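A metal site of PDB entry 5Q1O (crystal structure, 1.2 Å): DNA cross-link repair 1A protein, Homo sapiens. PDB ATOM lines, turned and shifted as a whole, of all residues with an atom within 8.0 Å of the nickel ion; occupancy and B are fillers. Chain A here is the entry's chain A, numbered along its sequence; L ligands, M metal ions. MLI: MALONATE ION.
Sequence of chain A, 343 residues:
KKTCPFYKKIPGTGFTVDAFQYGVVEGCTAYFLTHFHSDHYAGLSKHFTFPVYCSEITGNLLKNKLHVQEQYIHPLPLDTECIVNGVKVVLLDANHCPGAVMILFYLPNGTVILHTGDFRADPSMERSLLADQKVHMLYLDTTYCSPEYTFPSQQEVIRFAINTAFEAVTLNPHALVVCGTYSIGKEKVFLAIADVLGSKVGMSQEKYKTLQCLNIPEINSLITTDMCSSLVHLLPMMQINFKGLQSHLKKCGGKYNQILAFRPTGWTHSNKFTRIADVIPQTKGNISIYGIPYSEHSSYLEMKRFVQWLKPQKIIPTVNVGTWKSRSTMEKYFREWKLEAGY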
ATOM      1  N   ASP A  18     -25.683  -8.815  20.250  1.00  0.00           N
ATOM      2  CA  ASP A  18     -26.341  -8.424  21.529  1.00  0.00           C
ATOM      3  C   ASP A  18     -27.827  -8.029  21.326  1.00  0.00           C
ATOM      4  O   ASP A  18     -28.324  -7.032  21.893  1.00  0.00           O
ATOM      5  CB  ASP A  18     -25.505  -7.362  22.255  1.00  0.00           C
ATOM      6  CG  ASP A  18     -24.075  -7.846  22.605  1.00  0.00           C
ATOM      7  OD1 ASP A  18     -23.805  -9.086  22.480  1.00  0.00           O
ATOM      8  OD2 ASP A  18     -23.266  -6.970  23.048  1.00  0.00           O
ATOM      9  N   THR A  34     -21.536 -10.713  22.904  1.00  0.00           N
ATOM     10  CA  THR A  34     -20.180 -10.248  23.226  1.00  0.00           C
ATOM     11  C   THR A  34     -19.752 -10.623  24.649  1.00  0.00           C
ATOM     12  O   THR A  34     -18.560 -10.889  24.877  1.00  0.00           O
ATOM     13  CB  THR A  34     -19.990  -8.733  23.013  1.00  0.00           C
ATOM     14  OG1 THR A  34     -20.870  -7.995  23.894  1.00  0.00           O
ATOM     15  CG2 THR A  34     -20.231  -8.327  21.554  1.00  0.00           C
ATOM     16  N   HIS A  35     -20.698 -10.606  25.609  1.00  0.00           N
ATOM     17  CA  HIS A  35     -20.347 -10.873  27.004  1.00  0.00           C
ATOM     18  C   HIS A  35     -21.593 -11.056  27.853  1.00  0.00           C
ATOM     19  O   HIS A  35     -22.699 -10.608  27.467  1.00  0.00           O
ATOM     20  CB  HIS A  35     -19.441  -9.755  27.594  1.00  0.00           C
ATOM     21  CG  HIS A  35     -20.074  -8.385  27.779  1.00  0.00           C
ATOM     22  ND1 HIS A  35     -20.448  -7.542  26.742  1.00  0.00           N
ATOM     23  CD2 HIS A  35     -20.298  -7.677  28.918  1.00  0.00           C
ATOM     24  CE1 HIS A  35     -20.892  -6.396  27.261  1.00  0.00           C
ATOM     25  NE2 HIS A  35     -20.775  -6.445  28.554  1.00  0.00           N
ATOM     26  N   PHE A  36     -21.401 -11.647  29.023  1.00  0.00           N
ATOM     27  CA  PHE A  36     -22.528 -11.986  29.935  1.00  0.00           C
ATOM     28  C   PHE A  36     -22.847 -10.844  30.931  1.00  0.00           C
ATOM     29  O   PHE A  36     -22.647 -11.004  32.170  1.00  0.00           O
ATOM     30  CB  PHE A  36     -22.186 -13.303  30.662  1.00  0.00           C
ATOM     31  CG  PHE A  36     -23.393 -13.957  31.353  1.00  0.00           C
ATOM     32  CD1 PHE A  36     -24.348 -14.654  30.597  1.00  0.00           C
ATOM     33  CD2 PHE A  36     -23.548 -13.912  32.740  1.00  0.00           C
ATOM     34  CE1 PHE A  36     -25.449 -15.247  31.231  1.00  0.00           C
ATOM     35  CE2 PHE A  36     -24.663 -14.515  33.372  1.00  0.00           C
ATOM     36  CZ  PHE A  36     -25.586 -15.176  32.610  1.00  0.00           C
ATOM     37  N   HIS A  37     -23.335  -9.720  30.402  1.00  0.00           N
ATOM     38  CA  HIS A  37     -23.916  -8.622  31.205  1.00  0.00           C
ATOM     39  C   HIS A  37     -25.391  -8.491  30.782  1.00  0.00           C
ATOM     40  O   HIS A  37     -25.721  -8.579  29.575  1.00  0.00           O
ATOM     41  CB  HIS A  37     -23.170  -7.295  31.048  1.00  0.00           C
ATOM     42  CG  HIS A  37     -21.930  -7.168  31.892  1.00  0.00           C
ATOM     43  ND1 HIS A  37     -20.957  -6.216  31.671  1.00  0.00           N
ATOM     44  CD2 HIS A  37     -21.541  -7.870  32.991  1.00  0.00           C
ATOM     45  CE1 HIS A  37     -20.021  -6.339  32.597  1.00  0.00           C
ATOM     46  NE2 HIS A  37     -20.360  -7.313  33.421  1.00  0.00           N
ATOM     47  N   SER A  38     -26.277  -8.267  31.754  1.00  0.00           N
ATOM     48  CA  SER A  38     -27.748  -8.400  31.548  1.00  0.00           C
ATOM     49  C   SER A  38     -28.314  -7.470  30.464  1.00  0.00           C
ATOM     50  O   SER A  38     -29.201  -7.909  29.729  1.00  0.00           O
ATOM     51  CB  SER A  38     -28.513  -8.324  32.874  1.00  0.00           C
ATOM     52  OG  SER A  38     -28.345  -7.065  33.437  1.00  0.00           O
ATOM     53  N   ASP A  39     -27.792  -6.241  30.317  1.00  0.00           N
ATOM     54  CA  ASP A  39     -28.306  -5.347  29.233  1.00  0.00           C
ATOM     55  C   ASP A  39     -28.023  -5.957  27.822  1.00  0.00           C
ATOM     56  O   ASP A  39     -28.730  -5.605  26.851  1.00  0.00           O
ATOM     57  CB  ASP A  39     -27.706  -3.926  29.278  1.00  0.00           C
ATOM     58  CG  ASP A  39     -28.383  -2.978  30.310  1.00  0.00           C
ATOM     59  OD1 ASP A  39     -29.360  -3.345  30.973  1.00  0.00           O
ATOM     60  OD2 ASP A  39     -27.872  -1.846  30.454  1.00  0.00           O
ATOM     61  N   HIS A  40     -26.982  -6.817  27.714  1.00  0.00           N
ATOM     62  CA  HIS A  40     -26.578  -7.390  26.430  1.00  0.00           C
ATOM     63  C   HIS A  40     -27.226  -8.742  26.165  1.00  0.00           C
ATOM     64  O   HIS A  40     -27.604  -9.036  25.012  1.00  0.00           O
ATOM     65  CB  HIS A  40     -25.035  -7.483  26.386  1.00  0.00           C
ATOM     66  CG  HIS A  40     -24.376  -6.154  26.458  1.00  0.00           C
ATOM     67  ND1 HIS A  40     -23.873  -5.502  25.355  1.00  0.00           N
ATOM     68  CD2 HIS A  40     -24.206  -5.306  27.504  1.00  0.00           C
ATOM     69  CE1 HIS A  40     -23.440  -4.297  25.711  1.00  0.00           C
ATOM     70  NE2 HIS A  40     -23.623  -4.164  27.016  1.00  0.00           N
ATOM     71  N   HIS A  96     -12.605  -6.410  29.281  1.00  0.00           N
ATOM     72  CA  HIS A  96     -13.843  -5.951  29.996  1.00  0.00           C
ATOM     73  C   HIS A  96     -14.002  -6.895  31.177  1.00  0.00           C
ATOM     74  O   HIS A  96     -13.139  -6.889  32.051  1.00  0.00           O
ATOM     75  CB  HIS A  96     -15.030  -5.870  29.003  1.00  0.00           C
ATOM     76  CG  HIS A  96     -16.336  -5.344  29.565  1.00  0.00           C
ATOM     77  ND1 HIS A  96     -16.440  -4.146  30.220  1.00  0.00           N
ATOM     78  CD2 HIS A  96     -17.605  -5.854  29.519  1.00  0.00           C
ATOM     79  CE1 HIS A  96     -17.708  -3.939  30.581  1.00  0.00           C
ATOM     80  NE2 HIS A  96     -18.444  -4.955  30.150  1.00  0.00           N
ATOM     81  N   CYS A  97     -15.051  -7.723  31.218  1.00  0.00           N
ATOM     82  CA  CYS A  97     -15.241  -8.764  32.224  1.00  0.00           C
ATOM     83  C   CYS A  97     -14.799 -10.128  31.678  1.00  0.00           C
ATOM     84  O   CYS A  97     -14.542 -10.266  30.492  1.00  0.00           O
ATOM     85  CB  CYS A  97     -16.728  -8.790  32.629  1.00  0.00           C
ATOM     86  SG  CYS A  97     -17.884  -9.267  31.288  1.00  0.00           S
ATOM     87  N   ALA A 100     -15.497 -11.642  27.883  1.00  0.00           N
ATOM     88  CA  ALA A 100     -15.913 -10.574  26.970  1.00  0.00           C
ATOM     89  C   ALA A 100     -15.022 -10.493  25.755  1.00  0.00           C
ATOM     90  O   ALA A 100     -13.775 -10.531  25.868  1.00  0.00           O
ATOM     91  CB  ALA A 100     -15.929  -9.207  27.683  1.00  0.00           C
ATOM     92  N   GLY A 117     -17.890  -4.678  21.264  1.00  0.00           N
ATOM     93  CA  GLY A 117     -18.736  -4.980  22.424  1.00  0.00           C
ATOM     94  C   GLY A 117     -18.497  -3.895  23.477  1.00  0.00           C
ATOM     95  O   GLY A 117     -18.360  -2.722  23.128  1.00  0.00           O
ATOM     96  N   ASP A 118     -18.475  -4.287  24.757  1.00  0.00           N
ATOM     97  CA  ASP A 118     -17.939  -3.401  25.809  1.00  0.00           C
ATOM     98  C   ASP A 118     -16.427  -3.674  25.927  1.00  0.00           C
ATOM     99  O   ASP A 118     -15.998  -4.832  25.940  1.00  0.00           O
ATOM    100  CB  ASP A 118     -18.605  -3.652  27.162  1.00  0.00           C
ATOM    101  CG  ASP A 118     -20.002  -3.052  27.318  1.00  0.00           C
ATOM    102  OD1 ASP A 118     -20.434  -2.232  26.479  1.00  0.00           O
ATOM    103  OD2 ASP A 118     -20.653  -3.349  28.360  1.00  0.00           O
ATOM    104  N   PHE A 119     -15.618  -2.609  26.071  1.00  0.00           N
ATOM    105  CA  PHE A 119     -14.166  -2.819  26.154  1.00  0.00           C
ATOM    106  C   PHE A 119     -13.494  -1.729  26.983  1.00  0.00           C
ATOM    107  O   PHE A 119     -14.019  -0.611  27.107  1.00  0.00           O
ATOM    108  CB  PHE A 119     -13.503  -2.995  24.740  1.00  0.00           C
ATOM    109  CG  PHE A 119     -13.096  -1.719  23.972  1.00  0.00           C
ATOM    110  CD1 PHE A 119     -11.902  -1.686  23.230  1.00  0.00           C
ATOM    111  CD2 PHE A 119     -13.931  -0.591  23.894  1.00  0.00           C
ATOM    112  CE1 PHE A 119     -11.568  -0.589  22.452  1.00  0.00           C
ATOM    113  CE2 PHE A 119     -13.560   0.539  23.144  1.00  0.00           C
ATOM    114  CZ  PHE A 119     -12.381   0.521  22.410  1.00  0.00           C
ATOM    115  N   ASP A 141     -17.818   1.050  21.742  1.00  0.00           N
ATOM    116  CA  ASP A 141     -18.266   1.294  23.153  1.00  0.00           C
ATOM    117  C   ASP A 141     -17.830   2.717  23.537  1.00  0.00           C
ATOM    118  O   ASP A 141     -16.679   2.960  23.904  1.00  0.00           O
ATOM    119  CB  ASP A 141     -17.659   0.266  24.108  1.00  0.00           C
ATOM    120  CG  ASP A 141     -17.855   0.594  25.576  1.00  0.00           C
ATOM    121  OD1 ASP A 141     -18.698   1.498  25.875  1.00  0.00           O
ATOM    122  OD2 ASP A 141     -17.172  -0.080  26.416  1.00  0.00           O
ATOM    123  N   THR A 143     -19.138   4.534  26.121  1.00  0.00           N
ATOM    124  CA  THR A 143     -19.618   4.803  27.483  1.00  0.00           C
ATOM    125  C   THR A 143     -19.078   6.122  28.049  1.00  0.00           C
ATOM    126  O   THR A 143     -19.873   6.990  28.504  1.00  0.00           O
ATOM    127  CB  THR A 143     -19.298   3.619  28.443  1.00  0.00           C
ATOM    128  OG1 THR A 143     -19.997   2.426  28.008  1.00  0.00           O
ATOM    129  CG2 THR A 143     -19.727   3.885  29.859  1.00  0.00           C
ATOM    130  N   SER A 183     -22.856  -8.320  39.250  1.00  0.00           N
ATOM    131  CA  SER A 183     -22.587  -8.850  37.908  1.00  0.00           C
ATOM    132  C   SER A 183     -21.205  -9.489  37.920  1.00  0.00           C
ATOM    133  O   SER A 183     -20.454  -9.328  38.894  1.00  0.00           O
ATOM    134  CB  SER A 183     -22.623  -7.742  36.829  1.00  0.00           C
ATOM    135  OG  SER A 183     -21.570  -6.824  37.058  1.00  0.00           O
ATOM    136  N   ILE A 184     -20.857 -10.188  36.863  1.00  0.00           N
ATOM    137  CA  ILE A 184     -19.457 -10.599  36.667  1.00  0.00           C
ATOM    138  C   ILE A 184     -18.626  -9.345  36.282  1.00  0.00           C
ATOM    139  O   ILE A 184     -19.166  -8.280  35.873  1.00  0.00           O
ATOM    140  CB  ILE A 184     -19.252 -11.740  35.629  1.00  0.00           C
ATOM    141  CG1 ILE A 184     -19.616 -11.334  34.203  1.00  0.00           C
ATOM    142  CG2 ILE A 184     -20.007 -12.978  36.051  1.00  0.00           C
ATOM    143  CD1 ILE A 184     -19.139 -12.328  33.158  1.00  0.00           C
ATOM    144  N   GLU A 296     -14.061  -1.028  34.023  1.00  0.00           N
ATOM    145  CA  GLU A 296     -13.866  -1.998  32.912  1.00  0.00           C
ATOM    146  C   GLU A 296     -14.328  -1.409  31.555  1.00  0.00           C
ATOM    147  O   GLU A 296     -14.527  -2.153  30.571  1.00  0.00           O
ATOM    148  CB  GLU A 296     -14.461  -3.383  33.247  1.00  0.00           C
ATOM    149  CG  GLU A 296     -13.703  -4.087  34.383  1.00  0.00           C
ATOM    150  CD  GLU A 296     -14.101  -5.538  34.684  1.00  0.00           C
ATOM    151  OE1 GLU A 296     -15.259  -5.925  34.370  1.00  0.00           O
ATOM    152  OE2 GLU A 296     -13.252  -6.272  35.308  1.00  0.00           O
ATOM    153  N   HIS A 297     -14.408  -0.071  31.480  1.00  0.00           N
ATOM    154  CA  HIS A 297     -14.611   0.667  30.214  1.00  0.00           C
ATOM    155  C   HIS A 297     -13.445   1.656  29.989  1.00  0.00           C
ATOM    156  O   HIS A 297     -12.855   2.183  30.937  1.00  0.00           O
ATOM    157  CB  HIS A 297     -15.937   1.456  30.176  1.00  0.00           C
ATOM    158  CG  HIS A 297     -17.182   0.645  30.230  1.00  0.00           C
ATOM    159  ND1 HIS A 297     -17.773   0.065  29.134  1.00  0.00           N
ATOM    160  CD2 HIS A 297     -17.971   0.341  31.289  1.00  0.00           C
ATOM    161  CE1 HIS A 297     -18.893  -0.546  29.512  1.00  0.00           C
ATOM    162  NE2 HIS A 297     -19.015  -0.391  30.819  1.00  0.00           N
HETATM  163  C1  MLI L   1     -22.686  -3.213  32.067  1.00  0.00           C
HETATM  164  C2  MLI L   1     -21.341  -2.530  31.915  1.00  0.00           C
HETATM  165  C3  MLI L   1     -23.326  -3.628  30.750  1.00  0.00           C
HETATM  166  O6  MLI L   1     -21.056  -1.447  32.446  1.00  0.00           O
HETATM  167  O7  MLI L   1     -20.475  -3.164  31.303  1.00  0.00           O
HETATM  168  O8  MLI L   1     -24.541  -3.340  30.531  1.00  0.00           O
HETATM  169  O9  MLI L   1     -22.665  -4.345  29.981  1.00  0.00           O
HETATM  170 NI    NI M   1     -20.652  -4.799  30.006  1.00  0.00          NI
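OD2 of Asp 118 lies close to NE2 of His 40.
A ring nitrogen (ND1) of His 35 is in hydrogen-bond range of the side-chain hydroxyl of Thr 34.
NE2 of His 37 lies within hydrogen-bond range of O of Ile 184 (2.9 Å).
A ring nitrogen (ND1) of His 96 sits at hydrogen-bond distance from the backbone carbonyl oxygen of Glu 296 (2.8 Å).
O9 of the ligand binds the nickel ion.
O7 of the ligand binds the nickel ion (2.1 Å).
The nickel ion is bound by OD2 of Asp 118, at 2.2 Å.
NE2 of His 35 binds the nickel ion, at 2.2 Å.
ND1 of His 37 binds the nickel ion, at 2.2 Å.
The nickel ion is bound by a ring nitrogen (NE2) of His 96 (2.2 Å).
The nickel ion has six donor atoms within binding distance.
Of the 20 residues printed, 4 come within 4 Å of the nickel ion.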
